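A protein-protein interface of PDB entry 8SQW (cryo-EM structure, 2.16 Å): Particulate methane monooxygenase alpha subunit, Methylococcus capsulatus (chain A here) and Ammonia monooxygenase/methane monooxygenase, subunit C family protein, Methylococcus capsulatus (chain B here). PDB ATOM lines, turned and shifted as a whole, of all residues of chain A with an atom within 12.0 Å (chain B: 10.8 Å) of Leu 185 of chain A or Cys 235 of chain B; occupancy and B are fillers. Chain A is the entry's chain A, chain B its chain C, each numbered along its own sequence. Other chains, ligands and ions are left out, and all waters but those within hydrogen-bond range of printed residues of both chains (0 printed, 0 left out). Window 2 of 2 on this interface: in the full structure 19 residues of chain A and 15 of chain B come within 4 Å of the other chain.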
ATOM      1  N   PRO A 178      -6.060 -11.981  15.276  1.00  0.00           N
ATOM      2  CA  PRO A 178      -5.534 -12.804  14.181  1.00  0.00           C
ATOM      3  C   PRO A 178      -5.949 -12.254  12.823  1.00  0.00           C
ATOM      4  O   PRO A 178      -7.044 -11.714  12.656  1.00  0.00           O
ATOM      5  CB  PRO A 178      -6.143 -14.186  14.450  1.00  0.00           C
ATOM      6  CG  PRO A 178      -7.208 -13.966  15.487  1.00  0.00           C
ATOM      7  CD  PRO A 178      -6.738 -12.805  16.290  1.00  0.00           C
ATOM      8  N   ILE A 179      -5.056 -12.397  11.841  1.00  0.00           N
ATOM      9  CA  ILE A 179      -5.151 -11.608  10.617  1.00  0.00           C
ATOM     10  C   ILE A 179      -5.685 -12.397   9.428  1.00  0.00           C
ATOM     11  O   ILE A 179      -6.736 -12.061   8.876  1.00  0.00           O
ATOM     12  CB  ILE A 179      -3.785 -10.991  10.271  1.00  0.00           C
ATOM     13  CG1 ILE A 179      -3.261 -10.161  11.443  1.00  0.00           C
ATOM     14  CG2 ILE A 179      -3.885 -10.140   9.015  1.00  0.00           C
ATOM     15  CD1 ILE A 179      -1.790  -9.837  11.344  1.00  0.00           C
ATOM     16  N   PHE A 180      -4.967 -13.434   8.993  1.00  0.00           N
ATOM     17  CA  PHE A 180      -5.205 -13.969   7.655  1.00  0.00           C
ATOM     18  C   PHE A 180      -6.044 -15.243   7.627  1.00  0.00           C
ATOM     19  O   PHE A 180      -7.144 -15.244   7.070  1.00  0.00           O
ATOM     20  CB  PHE A 180      -3.861 -14.213   6.957  1.00  0.00           C
ATOM     21  CG  PHE A 180      -3.213 -12.961   6.449  1.00  0.00           C
ATOM     22  CD1 PHE A 180      -3.810 -12.217   5.446  1.00  0.00           C
ATOM     23  CD2 PHE A 180      -2.011 -12.526   6.975  1.00  0.00           C
ATOM     24  CE1 PHE A 180      -3.218 -11.063   4.978  1.00  0.00           C
ATOM     25  CE2 PHE A 180      -1.416 -11.370   6.512  1.00  0.00           C
ATOM     26  CZ  PHE A 180      -2.020 -10.638   5.511  1.00  0.00           C
ATOM     27  N   ILE A 181      -5.568 -16.321   8.238  1.00  0.00           N
ATOM     28  CA  ILE A 181      -6.171 -17.628   7.975  1.00  0.00           C
ATOM     29  C   ILE A 181      -7.480 -17.798   8.742  1.00  0.00           C
ATOM     30  O   ILE A 181      -8.475 -18.232   8.140  1.00  0.00           O
ATOM     31  CB  ILE A 181      -5.190 -18.772   8.280  1.00  0.00           C
ATOM     32  CG1 ILE A 181      -4.034 -18.757   7.276  1.00  0.00           C
ATOM     33  CG2 ILE A 181      -5.904 -20.104   8.193  1.00  0.00           C
ATOM     34  CD1 ILE A 181      -3.246 -20.047   7.226  1.00  0.00           C
ATOM     35  N   PRO A 182      -7.547 -17.512  10.050  1.00  0.00           N
ATOM     36  CA  PRO A 182      -8.857 -17.604  10.720  1.00  0.00           C
ATOM     37  C   PRO A 182      -9.901 -16.668  10.138  1.00  0.00           C
ATOM     38  O   PRO A 182     -11.069 -17.055  10.023  1.00  0.00           O
ATOM     39  CB  PRO A 182      -8.529 -17.261  12.182  1.00  0.00           C
ATOM     40  CG  PRO A 182      -7.233 -16.556  12.133  1.00  0.00           C
ATOM     41  CD  PRO A 182      -6.483 -17.169  11.009  1.00  0.00           C
ATOM     42  N   ARG A 183      -9.514 -15.454   9.742  1.00  0.00           N
ATOM     43  CA  ARG A 183     -10.482 -14.543   9.133  1.00  0.00           C
ATOM     44  C   ARG A 183     -10.939 -15.057   7.776  1.00  0.00           C
ATOM     45  O   ARG A 183     -12.124 -14.957   7.435  1.00  0.00           O
ATOM     46  CB  ARG A 183      -9.890 -13.138   9.009  1.00  0.00           C
ATOM     47  CG  ARG A 183      -9.760 -12.403  10.331  1.00  0.00           C
ATOM     48  CD  ARG A 183      -9.263 -10.981  10.145  1.00  0.00           C
ATOM     49  NE  ARG A 183     -10.345 -10.052   9.849  1.00  0.00           N
ATOM     50  CZ  ARG A 183     -10.997  -9.347  10.763  1.00  0.00           C
ATOM     51  NH1 ARG A 183     -10.713  -9.455  12.050  1.00  0.00           N
ATOM     52  NH2 ARG A 183     -11.956  -8.511  10.376  1.00  0.00           N
ATOM     53  N   LEU A 184     -10.015 -15.615   6.989  1.00  0.00           N
ATOM     54  CA  LEU A 184     -10.387 -16.208   5.709  1.00  0.00           C
ATOM     55  C   LEU A 184     -11.367 -17.358   5.905  1.00  0.00           C
ATOM     56  O   LEU A 184     -12.359 -17.471   5.176  1.00  0.00           O
ATOM     57  CB  LEU A 184      -9.133 -16.693   4.984  1.00  0.00           C
ATOM     58  CG  LEU A 184      -9.314 -17.542   3.727  1.00  0.00           C
ATOM     59  CD1 LEU A 184      -9.838 -16.695   2.582  1.00  0.00           C
ATOM     60  CD2 LEU A 184      -8.006 -18.215   3.346  1.00  0.00           C
ATOM     61  N   LEU A 185     -11.099 -18.221   6.888  1.00  0.00           N
ATOM     62  CA  LEU A 185     -11.993 -19.341   7.157  1.00  0.00           C
ATOM     63  C   LEU A 185     -13.359 -18.859   7.635  1.00  0.00           C
ATOM     64  O   LEU A 185     -14.388 -19.426   7.254  1.00  0.00           O
ATOM     65  CB  LEU A 185     -11.367 -20.278   8.190  1.00  0.00           C
ATOM     66  CG  LEU A 185     -10.165 -21.096   7.715  1.00  0.00           C
ATOM     67  CD1 LEU A 185      -9.536 -21.844   8.877  1.00  0.00           C
ATOM     68  CD2 LEU A 185     -10.567 -22.053   6.612  1.00  0.00           C
ATOM     69  N   MET A 186     -13.387 -17.824   8.475  1.00  0.00           N
ATOM     70  CA  MET A 186     -14.662 -17.283   8.936  1.00  0.00           C
ATOM     71  C   MET A 186     -15.464 -16.694   7.783  1.00  0.00           C
ATOM     72  O   MET A 186     -16.684 -16.882   7.712  1.00  0.00           O
ATOM     73  CB  MET A 186     -14.424 -16.228  10.016  1.00  0.00           C
ATOM     74  CG  MET A 186     -14.040 -16.803  11.366  1.00  0.00           C
ATOM     75  SD  MET A 186     -15.457 -17.466  12.255  1.00  0.00           S
ATOM     76  CE  MET A 186     -16.382 -15.965  12.571  1.00  0.00           C
ATOM     77  N   VAL A 187     -14.800 -15.973   6.878  1.00  0.00           N
ATOM     78  CA  VAL A 187     -15.507 -15.389   5.740  1.00  0.00           C
ATOM     79  C   VAL A 187     -16.020 -16.479   4.807  1.00  0.00           C
ATOM     80  O   VAL A 187     -17.153 -16.408   4.315  1.00  0.00           O
ATOM     81  CB  VAL A 187     -14.601 -14.388   5.003  1.00  0.00           C
ATOM     82  CG1 VAL A 187     -15.244 -13.950   3.699  1.00  0.00           C
ATOM     83  CG2 VAL A 187     -14.319 -13.180   5.883  1.00  0.00           C
ATOM     84  N   ASP A 188     -15.205 -17.506   4.551  1.00  0.00           N
ATOM     85  CA  ASP A 188     -15.605 -18.568   3.627  1.00  0.00           C
ATOM     86  C   ASP A 188     -16.730 -19.421   4.208  1.00  0.00           C
ATOM     87  O   ASP A 188     -17.808 -19.539   3.620  1.00  0.00           O
ATOM     88  CB  ASP A 188     -14.397 -19.437   3.270  1.00  0.00           C
ATOM     89  CG  ASP A 188     -13.418 -18.728   2.357  1.00  0.00           C
ATOM     90  OD1 ASP A 188     -13.868 -17.966   1.475  1.00  0.00           O
ATOM     91  OD2 ASP A 188     -12.197 -18.936   2.516  1.00  0.00           O
ATOM     92  N   ALA A 189     -16.489 -20.025   5.371  1.00  0.00           N
ATOM     93  CA  ALA A 189     -17.466 -20.920   5.980  1.00  0.00           C
ATOM     94  C   ALA A 189     -18.601 -20.125   6.607  1.00  0.00           C
ATOM     95  O   ALA A 189     -18.514 -19.706   7.764  1.00  0.00           O
ATOM     96  CB  ALA A 189     -16.800 -21.813   7.025  1.00  0.00           C
ATOM     97  N   GLY A 190     -19.672 -19.917   5.845  1.00  0.00           N
ATOM     98  CA  GLY A 190     -20.810 -19.165   6.325  1.00  0.00           C
ATOM     99  C   GLY A 190     -20.581 -17.668   6.257  1.00  0.00           C
ATOM    100  O   GLY A 190     -19.514 -17.177   5.886  1.00  0.00           O
ATOM    101  N   ARG A 191     -21.622 -16.931   6.630  1.00  0.00           N
ATOM    102  CA  ARG A 191     -21.521 -15.483   6.699  1.00  0.00           C
ATOM    103  C   ARG A 191     -20.572 -15.090   7.826  1.00  0.00           C
ATOM    104  O   ARG A 191     -20.554 -15.702   8.896  1.00  0.00           O
ATOM    105  CB  ARG A 191     -22.900 -14.869   6.933  1.00  0.00           C
ATOM    106  CG  ARG A 191     -23.780 -14.833   5.696  1.00  0.00           C
ATOM    107  CD  ARG A 191     -25.181 -14.362   6.046  1.00  0.00           C
ATOM    108  NE  ARG A 191     -26.038 -14.269   4.873  1.00  0.00           N
ATOM    109  CZ  ARG A 191     -27.329 -14.572   4.865  1.00  0.00           C
ATOM    110  NH1 ARG A 191     -27.946 -14.984   5.960  1.00  0.00           N
ATOM    111  NH2 ARG A 191     -28.014 -14.464   3.731  1.00  0.00           N
ATOM    112  N   ALA A 192     -19.769 -14.055   7.580  1.00  0.00           N
ATOM    113  CA  ALA A 192     -18.793 -13.698   8.599  1.00  0.00           C
ATOM    114  C   ALA A 192     -19.426 -12.843   9.683  1.00  0.00           C
ATOM    115  O   ALA A 192     -19.658 -13.325  10.796  1.00  0.00           O
ATOM    116  CB  ALA A 192     -17.614 -12.957   7.965  1.00  0.00           C
ATOM    117  N   ASP A 193     -19.733 -11.586   9.354  1.00  0.00           N
ATOM    118  CA  ASP A 193     -20.556 -10.683  10.167  1.00  0.00           C
ATOM    119  C   ASP A 193     -20.208 -10.745  11.656  1.00  0.00           C
ATOM    120  O   ASP A 193     -21.036 -10.471  12.526  1.00  0.00           O
ATOM    121  CB  ASP A 193     -22.040 -10.969   9.947  1.00  0.00           C
ATOM    122  CG  ASP A 193     -22.523 -10.515   8.584  1.00  0.00           C
ATOM    123  OD1 ASP A 193     -21.932  -9.564   8.031  1.00  0.00           O
ATOM    124  OD2 ASP A 193     -23.490 -11.110   8.068  1.00  0.00           O
ATOM    125  N   GLU A 194     -18.962 -11.113  11.951  1.00  0.00           N
ATOM    126  CA  GLU A 194     -18.553 -11.280  13.340  1.00  0.00           C
ATOM    127  C   GLU A 194     -17.186 -10.669  13.594  1.00  0.00           C
ATOM    128  O   GLU A 194     -16.853 -10.321  14.732  1.00  0.00           O
ATOM    129  CB  GLU A 194     -18.554 -12.762  13.719  1.00  0.00           C
ATOM    130  CG  GLU A 194     -19.918 -13.290  14.131  1.00  0.00           C
ATOM    131  CD  GLU A 194     -20.160 -14.713  13.666  1.00  0.00           C
ATOM    132  OE1 GLU A 194     -19.365 -15.601  14.034  1.00  0.00           O
ATOM    133  OE2 GLU A 194     -21.146 -14.942  12.934  1.00  0.00           O
ATOM    134  N   LEU A 195     -16.379 -10.543  12.541  1.00  0.00           N
ATOM    135  CA  LEU A 195     -15.044  -9.989  12.678  1.00  0.00           C
ATOM    136  C   LEU A 195     -15.020  -8.472  12.548  1.00  0.00           C
ATOM    137  O   LEU A 195     -13.986  -7.856  12.834  1.00  0.00           O
ATOM    138  CB  LEU A 195     -14.104 -10.621  11.650  1.00  0.00           C
ATOM    139  CG  LEU A 195     -14.254 -12.139  11.536  1.00  0.00           C
ATOM    140  CD1 LEU A 195     -14.968 -12.507  10.249  1.00  0.00           C
ATOM    141  CD2 LEU A 195     -12.926 -12.857  11.644  1.00  0.00           C
ATOM    142  N   LEU B 218      -1.351 -16.076  -2.419  1.00  0.00           N
ATOM    143  CA  LEU B 218      -1.321 -16.200  -0.970  1.00  0.00           C
ATOM    144  C   LEU B 218      -2.588 -16.851  -0.435  1.00  0.00           C
ATOM    145  O   LEU B 218      -2.530 -17.586   0.553  1.00  0.00           O
ATOM    146  CB  LEU B 218      -1.104 -14.835  -0.324  1.00  0.00           C
ATOM    147  CG  LEU B 218       0.333 -14.638   0.156  1.00  0.00           C
ATOM    148  CD1 LEU B 218       0.497 -13.278   0.787  1.00  0.00           C
ATOM    149  CD2 LEU B 218       0.725 -15.726   1.140  1.00  0.00           C
ATOM    150  N   THR B 219      -3.746 -16.595  -1.050  1.00  0.00           N
ATOM    151  CA  THR B 219      -4.910 -17.361  -0.607  1.00  0.00           C
ATOM    152  C   THR B 219      -4.765 -18.834  -0.974  1.00  0.00           C
ATOM    153  O   THR B 219      -5.210 -19.709  -0.215  1.00  0.00           O
ATOM    154  CB  THR B 219      -6.211 -16.774  -1.162  1.00  0.00           C
ATOM    155  OG1 THR B 219      -7.305 -17.644  -0.839  1.00  0.00           O
ATOM    156  CG2 THR B 219      -6.150 -16.608  -2.645  1.00  0.00           C
ATOM    157  N   GLN B 220      -4.103 -19.135  -2.095  1.00  0.00           N
ATOM    158  CA  GLN B 220      -3.792 -20.527  -2.414  1.00  0.00           C
ATOM    159  C   GLN B 220      -2.862 -21.144  -1.371  1.00  0.00           C
ATOM    160  O   GLN B 220      -3.071 -22.286  -0.946  1.00  0.00           O
ATOM    161  CB  GLN B 220      -3.174 -20.617  -3.806  1.00  0.00           C
ATOM    162  CG  GLN B 220      -4.185 -20.808  -4.920  1.00  0.00           C
ATOM    163  CD  GLN B 220      -3.525 -20.892  -6.277  1.00  0.00           C
ATOM    164  OE1 GLN B 220      -2.306 -20.788  -6.389  1.00  0.00           O
ATOM    165  NE2 GLN B 220      -4.326 -21.080  -7.318  1.00  0.00           N
ATOM    166  N   THR B 221      -1.831 -20.408  -0.948  1.00  0.00           N
ATOM    167  CA  THR B 221      -0.943 -20.930   0.093  1.00  0.00           C
ATOM    168  C   THR B 221      -1.656 -21.061   1.429  1.00  0.00           C
ATOM    169  O   THR B 221      -1.329 -21.955   2.213  1.00  0.00           O
ATOM    170  CB  THR B 221       0.306 -20.061   0.269  1.00  0.00           C
ATOM    171  OG1 THR B 221      -0.016 -18.899   1.044  1.00  0.00           O
ATOM    172  CG2 THR B 221       0.908 -19.663  -1.056  1.00  0.00           C
ATOM    173  N   PHE B 222      -2.611 -20.179   1.721  1.00  0.00           N
ATOM    174  CA  PHE B 222      -3.401 -20.318   2.939  1.00  0.00           C
ATOM    175  C   PHE B 222      -4.219 -21.602   2.906  1.00  0.00           C
ATOM    176  O   PHE B 222      -4.284 -22.338   3.898  1.00  0.00           O
ATOM    177  CB  PHE B 222      -4.312 -19.106   3.117  1.00  0.00           C
ATOM    178  CG  PHE B 222      -3.585 -17.853   3.492  1.00  0.00           C
ATOM    179  CD1 PHE B 222      -2.352 -17.912   4.115  1.00  0.00           C
ATOM    180  CD2 PHE B 222      -4.134 -16.612   3.218  1.00  0.00           C
ATOM    181  CE1 PHE B 222      -1.681 -16.758   4.459  1.00  0.00           C
ATOM    182  CE2 PHE B 222      -3.467 -15.456   3.558  1.00  0.00           C
ATOM    183  CZ  PHE B 222      -2.240 -15.529   4.178  1.00  0.00           C
ATOM    184  N   TYR B 223      -4.848 -21.888   1.765  1.00  0.00           N
ATOM    185  CA  TYR B 223      -5.588 -23.138   1.630  1.00  0.00           C
ATOM    186  C   TYR B 223      -4.661 -24.343   1.734  1.00  0.00           C
ATOM    187  O   TYR B 223      -5.018 -25.362   2.337  1.00  0.00           O
ATOM    188  CB  TYR B 223      -6.354 -23.158   0.308  1.00  0.00           C
ATOM    189  CG  TYR B 223      -7.590 -22.294   0.321  1.00  0.00           C
ATOM    190  CD1 TYR B 223      -8.368 -22.180   1.465  1.00  0.00           C
ATOM    191  CD2 TYR B 223      -7.982 -21.595  -0.812  1.00  0.00           C
ATOM    192  CE1 TYR B 223      -9.501 -21.390   1.483  1.00  0.00           C
ATOM    193  CE2 TYR B 223      -9.113 -20.802  -0.804  1.00  0.00           C
ATOM    194  CZ  TYR B 223      -9.867 -20.705   0.347  1.00  0.00           C
ATOM    195  OH  TYR B 223     -10.994 -19.918   0.354  1.00  0.00           O
ATOM    196  N   SER B 224      -3.465 -24.247   1.150  1.00  0.00           N
ATOM    197  CA  SER B 224      -2.494 -25.333   1.255  1.00  0.00           C
ATOM    198  C   SER B 224      -2.043 -25.543   2.693  1.00  0.00           C
ATOM    199  O   SER B 224      -1.857 -26.687   3.125  1.00  0.00           O
ATOM    200  CB  SER B 224      -1.293 -25.048   0.355  1.00  0.00           C
ATOM    201  OG  SER B 224      -0.103 -25.581   0.904  1.00  0.00           O
ATOM    202  N   PHE B 225      -1.848 -24.455   3.439  1.00  0.00           N
ATOM    203  CA  PHE B 225      -1.546 -24.551   4.861  1.00  0.00           C
ATOM    204  C   PHE B 225      -2.676 -25.235   5.615  1.00  0.00           C
ATOM    205  O   PHE B 225      -2.436 -26.104   6.460  1.00  0.00           O
ATOM    206  CB  PHE B 225      -1.312 -23.151   5.431  1.00  0.00           C
ATOM    207  CG  PHE B 225       0.132 -22.804   5.643  1.00  0.00           C
ATOM    208  CD1 PHE B 225       0.858 -23.389   6.664  1.00  0.00           C
ATOM    209  CD2 PHE B 225       0.759 -21.873   4.831  1.00  0.00           C
ATOM    210  CE1 PHE B 225       2.183 -23.060   6.870  1.00  0.00           C
ATOM    211  CE2 PHE B 225       2.084 -21.543   5.027  1.00  0.00           C
ATOM    212  CZ  PHE B 225       2.797 -22.137   6.049  1.00  0.00           C
ATOM    213  N   ALA B 226      -3.913 -24.856   5.316  1.00  0.00           N
ATOM    214  CA  ALA B 226      -5.093 -25.380   5.999  1.00  0.00           C
ATOM    215  C   ALA B 226      -5.679 -26.581   5.267  1.00  0.00           C
ATOM    216  O   ALA B 226      -6.871 -26.615   4.961  1.00  0.00           O
ATOM    217  CB  ALA B 226      -6.131 -24.277   6.152  1.00  0.00           C
ATOM    218  N   GLN B 227      -4.854 -27.586   4.973  1.00  0.00           N
ATOM    219  CA  GLN B 227      -5.344 -28.792   4.291  1.00  0.00           C
ATOM    220  C   GLN B 227      -5.683 -29.881   5.304  1.00  0.00           C
ATOM    221  O   GLN B 227      -6.846 -30.264   5.451  1.00  0.00           O
ATOM    222  CB  GLN B 227      -4.304 -29.285   3.282  1.00  0.00           C
ATOM    223  CG  GLN B 227      -4.317 -28.580   1.927  1.00  0.00           C
ATOM    224  CD  GLN B 227      -5.567 -28.862   1.108  1.00  0.00           C
ATOM    225  OE1 GLN B 227      -6.691 -28.624   1.550  1.00  0.00           O
ATOM    226  NE2 GLN B 227      -5.369 -29.379  -0.100  1.00  0.00           N
ATOM    227  N   GLY B 228      -4.674 -30.384   6.008  1.00  0.00           N
ATOM    228  CA  GLY B 228      -4.897 -31.366   7.051  1.00  0.00           C
ATOM    229  C   GLY B 228      -4.727 -30.786   8.435  1.00  0.00           C
ATOM    230  O   GLY B 228      -5.506 -31.078   9.348  1.00  0.00           O
ATOM    231  N   GLY B 229      -3.708 -29.948   8.598  1.00  0.00           N
ATOM    232  CA  GLY B 229      -3.439 -29.306   9.866  1.00  0.00           C
ATOM    233  C   GLY B 229      -4.051 -27.924   9.959  1.00  0.00           C
ATOM    234  O   GLY B 229      -3.453 -27.011  10.533  1.00  0.00           O
ATOM    235  N   LEU B 230      -5.243 -27.759   9.384  1.00  0.00           N
ATOM    236  CA  LEU B 230      -5.947 -26.488   9.478  1.00  0.00           C
ATOM    237  C   LEU B 230      -6.273 -26.122  10.917  1.00  0.00           C
ATOM    238  O   LEU B 230      -6.485 -24.940  11.210  1.00  0.00           O
ATOM    239  CB  LEU B 230      -7.230 -26.537   8.638  1.00  0.00           C
ATOM    240  CG  LEU B 230      -8.517 -27.179   9.163  1.00  0.00           C
ATOM    241  CD1 LEU B 230      -9.395 -26.162   9.886  1.00  0.00           C
ATOM    242  CD2 LEU B 230      -9.284 -27.844   8.030  1.00  0.00           C
ATOM    243  N   GLY B 231      -6.318 -27.105  11.810  1.00  0.00           N
ATOM    244  CA  GLY B 231      -6.557 -26.860  13.212  1.00  0.00           C
ATOM    245  C   GLY B 231      -6.497 -28.152  13.997  1.00  0.00           C
ATOM    246  O   GLY B 231      -5.667 -29.025  13.736  1.00  0.00           O
ATOM    247  N   GLN B 232      -7.415 -28.280  14.944  1.00  0.00           N
ATOM    248  CA  GLN B 232      -8.471 -27.292  15.101  1.00  0.00           C
ATOM    249  C   GLN B 232      -8.146 -26.261  16.172  1.00  0.00           C
ATOM    250  O   GLN B 232      -7.128 -26.371  16.858  1.00  0.00           O
ATOM    251  CB  GLN B 232      -9.799 -27.977  15.413  1.00  0.00           C
ATOM    252  CG  GLN B 232     -10.336 -28.807  14.259  1.00  0.00           C
ATOM    253  CD  GLN B 232     -10.161 -28.117  12.919  1.00  0.00           C
ATOM    254  OE1 GLN B 232      -9.272 -28.463  12.142  1.00  0.00           O
ATOM    255  NE2 GLN B 232     -11.008 -27.133  12.647  1.00  0.00           N
ATOM    256  N   SER B 233      -9.089 -25.325  16.335  1.00  0.00           N
ATOM    257  CA  SER B 233      -8.929 -23.992  16.913  1.00  0.00           C
ATOM    258  C   SER B 233      -9.592 -23.016  15.953  1.00  0.00           C
ATOM    259  O   SER B 233     -10.679 -22.496  16.223  1.00  0.00           O
ATOM    260  CB  SER B 233      -7.467 -23.590  17.118  1.00  0.00           C
ATOM    261  OG  SER B 233      -7.337 -22.183  17.223  1.00  0.00           O
ATOM    262  N   LEU B 234      -8.918 -22.758  14.837  1.00  0.00           N
ATOM    263  CA  LEU B 234      -9.498 -22.018  13.726  1.00  0.00           C
ATOM    264  C   LEU B 234     -10.818 -22.648  13.312  1.00  0.00           C
ATOM    265  O   LEU B 234     -10.875 -23.842  12.995  1.00  0.00           O
ATOM    266  CB  LEU B 234      -8.520 -22.000  12.545  1.00  0.00           C
ATOM    267  CG  LEU B 234      -7.173 -21.261  12.594  1.00  0.00           C
ATOM    268  CD1 LEU B 234      -6.309 -21.593  13.806  1.00  0.00           C
ATOM    269  CD2 LEU B 234      -6.401 -21.561  11.328  1.00  0.00           C
ATOM    270  N   CYS B 235     -11.880 -21.843  13.327  1.00  0.00           N
ATOM    271  CA  CYS B 235     -13.241 -22.312  13.054  1.00  0.00           C
ATOM    272  C   CYS B 235     -13.638 -23.428  14.019  1.00  0.00           C
ATOM    273  O   CYS B 235     -14.347 -24.375  13.661  1.00  0.00           O
ATOM    274  CB  CYS B 235     -13.392 -22.758  11.599  1.00  0.00           C
ATOM    275  SG  CYS B 235     -13.895 -21.444  10.464  1.00  0.00           S
ATOM    276  N   GLU B 236     -13.173 -23.308  15.259  1.00  0.00           N
ATOM    277  CA  GLU B 236     -13.574 -24.210  16.335  1.00  0.00           C
ATOM    278  C   GLU B 236     -13.258 -23.594  17.693  1.00  0.00           C
ATOM    279  O   GLU B 236     -14.025 -22.781  18.209  1.00  0.00           O
ATOM    280  CB  GLU B 236     -12.882 -25.570  16.210  1.00  0.00           C
ATOM    281  CG  GLU B 236     -13.767 -26.731  16.643  1.00  0.00           C
ATOM    282  CD  GLU B 236     -13.218 -28.084  16.232  1.00  0.00           C
ATOM    283  OE1 GLU B 236     -12.394 -28.643  16.987  1.00  0.00           O
ATOM    284  OE2 GLU B 236     -13.606 -28.586  15.157  1.00  0.00           O
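Hydrophobic or aromatic side chains of chain B that line the printed part of chain A: Phe 222, Tyr 223 and Leu 234.
Among the printed residues, 8 pairs touch across the chains.
Ile 181 of chain A touches just these residues of chain B: Phe 222 (3.7 Å) and Leu 234 (3.5 Å).
Leu 184 of chain A touches two residues of chain B.
Of chain B, only Leu 234 (3.8 Å) and Cys 235 (3.6 Å) come within 4 Å of Leu 185 of chain A.
No residue of chain B comes within 4 Å of Met 186 of chain A.
Ala 189 of chain A touches none of the printed residues of chain B.
Of the printed residues of chain A, Phe 222 of chain B touches Phe 180 (3.5 Å), Ile 181 (3.7 Å) and Leu 184 (3.8 Å).
Of the printed residues of chain A, Tyr 223 of chain B touches Leu 184 and Asp 188.
No residue of chain A comes within 4 Å of Ala 226 of chain B.
Leu 230 of chain B touches none of the printed residues of chain A.
No residue of chain A comes within 4 Å of Gln 232 of chain B.
No residue of chain A comes within 4 Å of Ser 233 of chain B.
Printed residues of chain A within 4 Å of Leu 234 of chain B: Ile 181 (3.5 Å) and Leu 185 (3.8 Å).
Cys 235 of chain B touches one residue of chain A.
The nearest residue of chain B that does not touch Leu 185 of chain A is Leu 230 of chain B (4.4 Å).
The nearest printed residue of chain A that does not touch Phe 222 of chain B is Leu 185 of chain A (6.9 Å).
The backbone carbonyl oxygen (O) of Leu 234 of chain B sits at hydrogen-bond distance from the side-chain amide nitrogen (NE2) of Gln 232 of chain B (3.3 Å).
CB of Phe 180 of chain A touches CZ of Phe 222 of chain B, 3.5 Å away.
CD1 of Phe 222 of chain B touches CG1 of Ile 181 of chain A, at 3.7 Å.
CD2 of Leu 234 of chain B touches CG2 of Ile 181 of chain A (3.5 Å).
CD2 of Leu 184 of chain A touches CB of Phe 222 of chain B (3.8 Å).
CE1 of Tyr 223 of chain B touches CD2 of Leu 184 of chain A (3.97 Å).
Leu 234 of chain B touches Leu 185 of chain A (CB to CD1, 3.8 Å).
CB of Leu 185 of chain A touches SG of Cys 235 of chain B, at 3.6 Å.
The side-chain carboxylate of Asp 188 of chain A sits at hydrogen-bond distance from the side-chain hydroxyl of Tyr 223 of chain B, 2.7 Å away.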
